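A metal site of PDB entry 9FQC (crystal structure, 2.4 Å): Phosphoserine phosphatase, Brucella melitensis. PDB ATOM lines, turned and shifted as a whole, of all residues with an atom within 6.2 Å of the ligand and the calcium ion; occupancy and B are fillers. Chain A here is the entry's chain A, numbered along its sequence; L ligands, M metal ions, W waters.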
ATOM      1  N   ASP A  98     -17.295 -10.073 -15.738  1.00  0.00           N
ATOM      2  CA  ASP A  98     -17.104  -9.651 -17.116  1.00  0.00           C
ATOM      3  C   ASP A  98     -15.623  -9.496 -17.438  1.00  0.00           C
ATOM      4  O   ASP A  98     -14.809  -9.211 -16.557  1.00  0.00           O
ATOM      5  CB  ASP A  98     -17.830  -8.322 -17.291  1.00  0.00           C
ATOM      6  CG  ASP A  98     -17.649  -7.738 -18.638  1.00  0.00           C
ATOM      7  OD1 ASP A  98     -18.013  -8.401 -19.637  1.00  0.00           O
ATOM      8  OD2 ASP A  98     -17.150  -6.604 -18.708  1.00  0.00           O
ATOM      9  N   MET A  99     -15.253  -9.682 -18.716  1.00  0.00           N
ATOM     10  CA  MET A  99     -13.840  -9.479 -19.050  1.00  0.00           C
ATOM     11  C   MET A  99     -13.529  -8.107 -19.659  1.00  0.00           C
ATOM     12  O   MET A  99     -12.746  -7.352 -19.081  1.00  0.00           O
ATOM     13  CB  MET A  99     -13.299 -10.547 -20.014  1.00  0.00           C
ATOM     14  CG  MET A  99     -11.894 -10.164 -20.512  1.00  0.00           C
ATOM     15  SD  MET A  99     -10.998 -11.433 -21.424  1.00  0.00           S
ATOM     16  CE  MET A  99     -11.821 -11.238 -23.035  1.00  0.00           C
ATOM     17  N   ASP A 100     -14.095  -7.793 -20.827  1.00  0.00           N
ATOM     18  CA  ASP A 100     -13.703  -6.603 -21.575  1.00  0.00           C
ATOM     19  C   ASP A 100     -14.108  -5.325 -20.848  1.00  0.00           C
ATOM     20  O   ASP A 100     -15.277  -5.162 -20.459  1.00  0.00           O
ATOM     21  CB  ASP A 100     -14.314  -6.607 -22.988  1.00  0.00           C
ATOM     22  CG  ASP A 100     -13.496  -7.418 -23.986  1.00  0.00           C
ATOM     23  OD1 ASP A 100     -12.470  -8.042 -23.637  1.00  0.00           O
ATOM     24  OD2 ASP A 100     -13.876  -7.433 -25.166  1.00  0.00           O
ATOM     25  N   SER A 101     -13.148  -4.415 -20.693  1.00  0.00           N
ATOM     26  CA  SER A 101     -13.283  -3.143 -19.996  1.00  0.00           C
ATOM     27  C   SER A 101     -13.538  -3.305 -18.512  1.00  0.00           C
ATOM     28  O   SER A 101     -13.766  -2.304 -17.833  1.00  0.00           O
ATOM     29  CB  SER A 101     -14.376  -2.259 -20.616  1.00  0.00           C
ATOM     30  OG  SER A 101     -14.016  -1.879 -21.921  1.00  0.00           O
ATOM     31  N   THR A 102     -13.515  -4.524 -17.990  1.00  0.00           N
ATOM     32  CA  THR A 102     -13.667  -4.787 -16.563  1.00  0.00           C
ATOM     33  C   THR A 102     -12.387  -5.356 -15.970  1.00  0.00           C
ATOM     34  O   THR A 102     -11.714  -4.670 -15.193  1.00  0.00           O
ATOM     35  CB  THR A 102     -14.867  -5.715 -16.324  1.00  0.00           C
ATOM     36  OG1 THR A 102     -16.083  -5.067 -16.740  1.00  0.00           O
ATOM     37  CG2 THR A 102     -15.018  -6.094 -14.855  1.00  0.00           C
ATOM     38  N   GLU A 107     -11.206  -3.489 -25.266  1.00  0.00           N
ATOM     39  CA  GLU A 107     -12.180  -4.339 -25.943  1.00  0.00           C
ATOM     40  C   GLU A 107     -11.414  -5.165 -26.964  1.00  0.00           C
ATOM     41  O   GLU A 107     -10.919  -4.619 -27.953  1.00  0.00           O
ATOM     42  CB  GLU A 107     -13.270  -3.506 -26.611  1.00  0.00           C
ATOM     43  CG  GLU A 107     -14.010  -2.593 -25.663  1.00  0.00           C
ATOM     44  CD  GLU A 107     -15.124  -3.314 -24.934  1.00  0.00           C
ATOM     45  OE1 GLU A 107     -15.498  -4.425 -25.356  1.00  0.00           O
ATOM     46  OE2 GLU A 107     -15.609  -2.787 -23.914  1.00  0.00           O
ATOM     47  N   CYS A 108     -11.305  -6.474 -26.736  1.00  0.00           N
ATOM     48  CA  CYS A 108     -10.512  -7.292 -27.645  1.00  0.00           C
ATOM     49  C   CYS A 108     -11.020  -7.188 -29.072  1.00  0.00           C
ATOM     50  O   CYS A 108     -10.217  -7.181 -30.009  1.00  0.00           O
ATOM     51  CB  CYS A 108     -10.522  -8.749 -27.193  1.00  0.00           C
ATOM     52  SG  CYS A 108      -9.939  -8.982 -25.525  1.00  0.00           S
ATOM     53  N   ILE A 109     -12.332  -7.064 -29.247  1.00  0.00           N
ATOM     54  CA  ILE A 109     -12.893  -6.969 -30.592  1.00  0.00           C
ATOM     55  C   ILE A 109     -12.448  -5.677 -31.285  1.00  0.00           C
ATOM     56  O   ILE A 109     -12.150  -5.680 -32.482  1.00  0.00           O
ATOM     57  CB  ILE A 109     -14.428  -7.100 -30.529  1.00  0.00           C
ATOM     58  CG1 ILE A 109     -15.053  -6.900 -31.903  1.00  0.00           C
ATOM     59  CG2 ILE A 109     -15.024  -6.098 -29.553  1.00  0.00           C
ATOM     60  CD1 ILE A 109     -15.030  -8.140 -32.766  1.00  0.00           C
ATOM     61  N   THR A 126     -19.383  -1.265 -30.961  1.00  0.00           N
ATOM     62  CA  THR A 126     -19.185  -1.780 -29.613  1.00  0.00           C
ATOM     63  C   THR A 126     -19.782  -0.848 -28.563  1.00  0.00           C
ATOM     64  O   THR A 126     -20.458  -1.301 -27.631  1.00  0.00           O
ATOM     65  CB  THR A 126     -17.689  -1.972 -29.359  1.00  0.00           C
ATOM     66  OG1 THR A 126     -17.177  -2.888 -30.321  1.00  0.00           O
ATOM     67  CG2 THR A 126     -17.426  -2.522 -27.967  1.00  0.00           C
ATOM     68  N   ALA A 129     -23.416  -1.324 -28.510  1.00  0.00           N
ATOM     69  CA  ALA A 129     -23.809  -2.607 -27.937  1.00  0.00           C
ATOM     70  C   ALA A 129     -23.674  -2.604 -26.422  1.00  0.00           C
ATOM     71  O   ALA A 129     -24.569  -3.074 -25.704  1.00  0.00           O
ATOM     72  CB  ALA A 129     -22.968  -3.741 -28.545  1.00  0.00           C
ATOM     73  N   MET A 130     -22.556  -2.091 -25.907  1.00  0.00           N
ATOM     74  CA  MET A 130     -22.390  -2.068 -24.456  1.00  0.00           C
ATOM     75  C   MET A 130     -23.300  -1.051 -23.783  1.00  0.00           C
ATOM     76  O   MET A 130     -23.581  -1.188 -22.588  1.00  0.00           O
ATOM     77  CB  MET A 130     -20.926  -1.824 -24.112  1.00  0.00           C
ATOM     78  CG  MET A 130     -19.985  -2.924 -24.648  1.00  0.00           C
ATOM     79  SD  MET A 130     -20.154  -4.573 -23.887  1.00  0.00           S
ATOM     80  CE  MET A 130     -21.448  -5.366 -24.859  1.00  0.00           C
ATOM     81  N   PHE A 136     -26.850  -7.737 -28.339  1.00  0.00           N
ATOM     82  CA  PHE A 136     -25.461  -8.171 -28.373  1.00  0.00           C
ATOM     83  C   PHE A 136     -25.165  -9.054 -29.582  1.00  0.00           C
ATOM     84  O   PHE A 136     -24.131  -8.880 -30.242  1.00  0.00           O
ATOM     85  CB  PHE A 136     -25.075  -8.897 -27.093  1.00  0.00           C
ATOM     86  CG  PHE A 136     -23.653  -9.357 -27.096  1.00  0.00           C
ATOM     87  CD1 PHE A 136     -22.635  -8.458 -26.819  1.00  0.00           C
ATOM     88  CD2 PHE A 136     -23.333 -10.674 -27.429  1.00  0.00           C
ATOM     89  CE1 PHE A 136     -21.306  -8.853 -26.836  1.00  0.00           C
ATOM     90  CE2 PHE A 136     -21.999 -11.082 -27.440  1.00  0.00           C
ATOM     91  CZ  PHE A 136     -20.981 -10.166 -27.146  1.00  0.00           C
ATOM     92  N   LEU A 140     -22.364  -8.500 -32.448  1.00  0.00           N
ATOM     93  CA  LEU A 140     -21.159  -9.318 -32.520  1.00  0.00           C
ATOM     94  C   LEU A 140     -20.903  -9.847 -33.931  1.00  0.00           C
ATOM     95  O   LEU A 140     -19.775  -9.776 -34.428  1.00  0.00           O
ATOM     96  CB  LEU A 140     -21.231 -10.486 -31.535  1.00  0.00           C
ATOM     97  CG  LEU A 140     -19.973 -11.327 -31.349  1.00  0.00           C
ATOM     98  CD1 LEU A 140     -18.797 -10.458 -30.875  1.00  0.00           C
ATOM     99  CD2 LEU A 140     -20.201 -12.480 -30.381  1.00  0.00           C
ATOM    100  N   ARG A 143     -19.609  -7.104 -36.206  1.00  0.00           N
ATOM    101  CA  ARG A 143     -18.220  -6.725 -35.962  1.00  0.00           C
ATOM    102  C   ARG A 143     -17.251  -7.823 -36.403  1.00  0.00           C
ATOM    103  O   ARG A 143     -16.231  -7.537 -37.035  1.00  0.00           O
ATOM    104  CB  ARG A 143     -18.019  -6.399 -34.492  1.00  0.00           C
ATOM    105  CG  ARG A 143     -18.621  -5.063 -34.129  1.00  0.00           C
ATOM    106  CD  ARG A 143     -18.541  -4.823 -32.637  1.00  0.00           C
ATOM    107  NE  ARG A 143     -19.469  -5.687 -31.911  1.00  0.00           N
ATOM    108  CZ  ARG A 143     -19.417  -5.890 -30.597  1.00  0.00           C
ATOM    109  NH1 ARG A 143     -18.494  -5.313 -29.839  1.00  0.00           N
ATOM    110  NH2 ARG A 143     -20.305  -6.702 -30.029  1.00  0.00           N
ATOM    111  N   VAL A 186     -16.419 -14.572 -17.334  1.00  0.00           N
ATOM    112  CA  VAL A 186     -17.512 -14.944 -18.227  1.00  0.00           C
ATOM    113  C   VAL A 186     -17.758 -13.760 -19.183  1.00  0.00           C
ATOM    114  O   VAL A 186     -18.176 -12.679 -18.750  1.00  0.00           O
ATOM    115  CB  VAL A 186     -18.776 -15.303 -17.435  1.00  0.00           C
ATOM    116  CG1 VAL A 186     -19.952 -15.532 -18.369  1.00  0.00           C
ATOM    117  CG2 VAL A 186     -18.518 -16.514 -16.549  1.00  0.00           C
ATOM    118  N   SER A 187     -17.545 -13.995 -20.477  1.00  0.00           N
ATOM    119  CA  SER A 187     -17.345 -12.914 -21.429  1.00  0.00           C
ATOM    120  C   SER A 187     -18.115 -13.187 -22.726  1.00  0.00           C
ATOM    121  O   SER A 187     -18.272 -14.343 -23.145  1.00  0.00           O
ATOM    122  CB  SER A 187     -15.843 -12.733 -21.703  1.00  0.00           C
ATOM    123  OG  SER A 187     -15.593 -11.933 -22.835  1.00  0.00           O
ATOM    124  N   GLY A 188     -18.592 -12.105 -23.340  1.00  0.00           N
ATOM    125  CA  GLY A 188     -19.092 -12.157 -24.694  1.00  0.00           C
ATOM    126  C   GLY A 188     -18.004 -12.095 -25.748  1.00  0.00           C
ATOM    127  O   GLY A 188     -18.293 -12.223 -26.931  1.00  0.00           O
ATOM    128  N   GLY A 189     -16.752 -11.895 -25.306  1.00  0.00           N
ATOM    129  CA  GLY A 189     -15.584 -11.979 -26.181  1.00  0.00           C
ATOM    130  C   GLY A 189     -15.195 -13.399 -26.498  1.00  0.00           C
ATOM    131  O   GLY A 189     -16.041 -14.299 -26.574  1.00  0.00           O
ATOM    132  N   PHE A 190     -13.886 -13.633 -26.678  1.00  0.00           N
ATOM    133  CA  PHE A 190     -13.440 -14.850 -27.347  1.00  0.00           C
ATOM    134  C   PHE A 190     -12.550 -15.724 -26.474  1.00  0.00           C
ATOM    135  O   PHE A 190     -11.672 -15.226 -25.742  1.00  0.00           O
ATOM    136  CB  PHE A 190     -12.725 -14.492 -28.645  1.00  0.00           C
ATOM    137  CG  PHE A 190     -13.509 -13.514 -29.473  1.00  0.00           C
ATOM    138  CD1 PHE A 190     -14.763 -13.848 -29.966  1.00  0.00           C
ATOM    139  CD2 PHE A 190     -13.027 -12.231 -29.701  1.00  0.00           C
ATOM    140  CE1 PHE A 190     -15.513 -12.941 -30.705  1.00  0.00           C
ATOM    141  CE2 PHE A 190     -13.753 -11.318 -30.442  1.00  0.00           C
ATOM    142  CZ  PHE A 190     -15.013 -11.681 -30.942  1.00  0.00           C
ATOM    143  N   LYS A 232     -24.967 -15.252 -19.779  1.00  0.00           N
ATOM    144  CA  LYS A 232     -24.255 -14.985 -18.533  1.00  0.00           C
ATOM    145  C   LYS A 232     -25.118 -15.352 -17.329  1.00  0.00           C
ATOM    146  O   LYS A 232     -24.605 -15.875 -16.334  1.00  0.00           O
ATOM    147  CB  LYS A 232     -23.802 -13.521 -18.457  1.00  0.00           C
ATOM    148  CG  LYS A 232     -22.848 -13.097 -19.585  1.00  0.00           C
ATOM    149  CD  LYS A 232     -21.967 -11.902 -19.205  1.00  0.00           C
ATOM    150  CE  LYS A 232     -21.116 -11.431 -20.397  1.00  0.00           C
ATOM    151  NZ  LYS A 232     -19.857 -10.688 -19.989  1.00  0.00           N
ATOM    152  N   GLY A 254     -19.680  -6.003 -13.833  1.00  0.00           N
ATOM    153  CA  GLY A 254     -19.566  -5.735 -15.245  1.00  0.00           C
ATOM    154  C   GLY A 254     -19.731  -4.258 -15.509  1.00  0.00           C
ATOM    155  O   GLY A 254     -20.045  -3.474 -14.605  1.00  0.00           O
ATOM    156  N   ASP A 255     -19.528  -3.887 -16.777  1.00  0.00           N
ATOM    157  CA  ASP A 255     -19.660  -2.511 -17.254  1.00  0.00           C
ATOM    158  C   ASP A 255     -20.722  -2.318 -18.327  1.00  0.00           C
ATOM    159  O   ASP A 255     -21.034  -1.175 -18.648  1.00  0.00           O
ATOM    160  CB  ASP A 255     -18.326  -2.021 -17.827  1.00  0.00           C
ATOM    161  CG  ASP A 255     -18.003  -2.676 -19.168  1.00  0.00           C
ATOM    162  OD1 ASP A 255     -17.985  -3.918 -19.219  1.00  0.00           O
ATOM    163  OD2 ASP A 255     -17.793  -1.983 -20.176  1.00  0.00           O
ATOM    164  N   GLY A 256     -21.244  -3.398 -18.915  1.00  0.00           N
ATOM    165  CA  GLY A 256     -22.011  -3.303 -20.136  1.00  0.00           C
ATOM    166  C   GLY A 256     -23.428  -3.865 -20.002  1.00  0.00           C
ATOM    167  O   GLY A 256     -23.763  -4.570 -19.054  1.00  0.00           O
ATOM    168  N   ASN A 258     -24.856  -6.228 -21.608  1.00  0.00           N
ATOM    169  CA  ASN A 258     -24.864  -7.689 -21.562  1.00  0.00           C
ATOM    170  C   ASN A 258     -24.514  -8.253 -20.183  1.00  0.00           C
ATOM    171  O   ASN A 258     -24.602  -9.475 -20.018  1.00  0.00           O
ATOM    172  CB  ASN A 258     -23.900  -8.251 -22.625  1.00  0.00           C
ATOM    173  CG  ASN A 258     -22.461  -7.834 -22.362  1.00  0.00           C
ATOM    174  OD1 ASN A 258     -22.227  -6.741 -21.842  1.00  0.00           O
ATOM    175  ND2 ASN A 258     -21.495  -8.671 -22.750  1.00  0.00           N
ATOM    176  N   ASP A 259     -24.116  -7.443 -19.213  1.00  0.00           N
ATOM    177  CA  ASP A 259     -23.883  -7.934 -17.866  1.00  0.00           C
ATOM    178  C   ASP A 259     -25.072  -7.722 -16.940  1.00  0.00           C
ATOM    179  O   ASP A 259     -25.033  -8.176 -15.791  1.00  0.00           O
ATOM    180  CB  ASP A 259     -22.661  -7.273 -17.225  1.00  0.00           C
ATOM    181  CG  ASP A 259     -21.405  -7.449 -18.055  1.00  0.00           C
ATOM    182  OD1 ASP A 259     -21.119  -8.611 -18.393  1.00  0.00           O
ATOM    183  OD2 ASP A 259     -20.713  -6.428 -18.335  1.00  0.00           O
ATOM    184  N   LYS A 275     -21.250   1.970 -18.434  1.00  0.00           N
ATOM    185  CA  LYS A 275     -21.874   2.814 -19.447  1.00  0.00           C
ATOM    186  C   LYS A 275     -23.043   3.622 -18.859  1.00  0.00           C
ATOM    187  O   LYS A 275     -23.705   3.183 -17.906  1.00  0.00           O
ATOM    188  CB  LYS A 275     -22.309   1.949 -20.629  1.00  0.00           C
ATOM    189  CG  LYS A 275     -21.245   0.960 -21.078  1.00  0.00           C
ATOM    190  CD  LYS A 275     -19.947   1.634 -21.517  1.00  0.00           C
ATOM    191  CE  LYS A 275     -18.968   0.648 -22.161  1.00  0.00           C
ATOM    192  NZ  LYS A 275     -17.694   0.508 -21.385  1.00  0.00           N
HETATM  193  N1  LIG L   1     -17.382  -6.204 -24.726  1.00  0.00           N
HETATM  194  C1  LIG L   1     -17.307  -7.295 -25.716  1.00  0.00           C
HETATM  195  C2  LIG L   1     -17.842  -8.605 -25.084  1.00  0.00           C
HETATM  196  O1  LIG L   1     -16.898  -8.989 -24.158  1.00  0.00           O
HETATM  197  C3  LIG L   1     -18.102  -6.953 -26.973  1.00  0.00           C
HETATM  198  O2  LIG L   1     -18.682  -5.867 -27.100  1.00  0.00           O
HETATM  199  O3  LIG L   1     -18.126  -7.870 -27.869  1.00  0.00           O
HETATM  200  P1  LIG L   1     -17.300  -8.772 -22.429  1.00  0.00           P
HETATM  201  O4  LIG L   1     -16.111  -9.477 -21.765  1.00  0.00           O
HETATM  202  O5  LIG L   1     -17.422  -7.267 -22.295  1.00  0.00           O
HETATM  203  O6  LIG L   1     -18.655  -9.511 -22.355  1.00  0.00           O
HETATM  204 CA    CA M   1     -17.570  -5.585 -20.748  1.00  0.00          CA
HETATM  205  O   HOH W   1     -19.870  -6.010 -20.693  1.00  0.00           O
HETATM  206  O   HOH W   2     -17.556  -3.822 -22.259  1.00  0.00           O
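Within 4 Å of the calcium ion: Asp 98, Asp 100 and Asp 255.
The side-chain amide oxygen (OD1) of Asn 258 lies close to the side-chain sulfur (SD) of Met 130. OD2 of Asp 98 sits close to OG1 of Thr 102. The backbone carbonyl oxygen of Val 186 is in hydrogen-bond range of the side-chain amino group of Lys 232. The backbone NH of Asp 255 sits at hydrogen-bond distance from the side-chain carboxylate of Asp 259 (3.2 Å). NZ of Lys 275 lies within salt-bridge range of OD2 of Asp 255 (2.8 Å). The side-chain amino group (NZ) of Lys 232 is in salt-bridge range of the side-chain carboxylate (OD1) of Asp 259, at 2.9 Å. The side-chain hydroxyl (OG1) of Thr 102 lies close to the side-chain carboxylate (OD1) of Asp 255 (3.3 Å). The side-chain hydroxyl (OG) of Ser 187 sits at hydrogen-bond distance from the backbone NH (N) of Gly 189.
The calcium ion is bound by O5 of the ligand, OD1 of Asp 255, OD2 of Asp 98, water W2, water W1 and O of Asp 100. The calcium ion has six donor atoms within binding distance. Slightly farther from the calcium ion lies OD1 of Asp 98 (3.1 Å).
An oxygen (O6) of the ligand is in salt-bridge range of the side-chain amino group of Lys 232. An oxygen (O1) of the ligand is in hydrogen-bond range of the backbone NH of Gly 189 (3.1 Å). OE1 of Glu 107 lies within salt-bridge range of N1 of the ligand (2.7 Å). The guanidinium group of Arg 143 is in salt-bridge range of an oxygen (O2) of the ligand. OD2 of Asp 100 lies within salt-bridge range of N1 of the ligand (3.7 Å). The backbone NH (N) of Met 99 sits at hydrogen-bond distance from an oxygen (O4) of the ligand (3.2 Å). The side-chain sulfur of Met 130 sits at hydrogen-bond distance from a nitrogen (N1) of the ligand, at 3.3 Å. O6 of the ligand sits at hydrogen-bond distance from N of Gly 188, at 2.8 Å. An oxygen (O4) of the ligand sits at hydrogen-bond distance from the backbone NH (N) of Asp 100 (2.8 Å). O4 of the ligand sits at hydrogen-bond distance from OG of Ser 187 (2.7 Å). ND2 of Asn 258 lies within hydrogen-bond range of O6 of the ligand.
Residues that only touch the ligand: Phe 136 (3.5 Å), Thr 126 (3.7 Å) and Ile 109 (3.9 Å). Hydrophobic or aromatic side chains within 4 Å of the ligand: Met 99, Ile 109, Met 130 and Phe 136.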
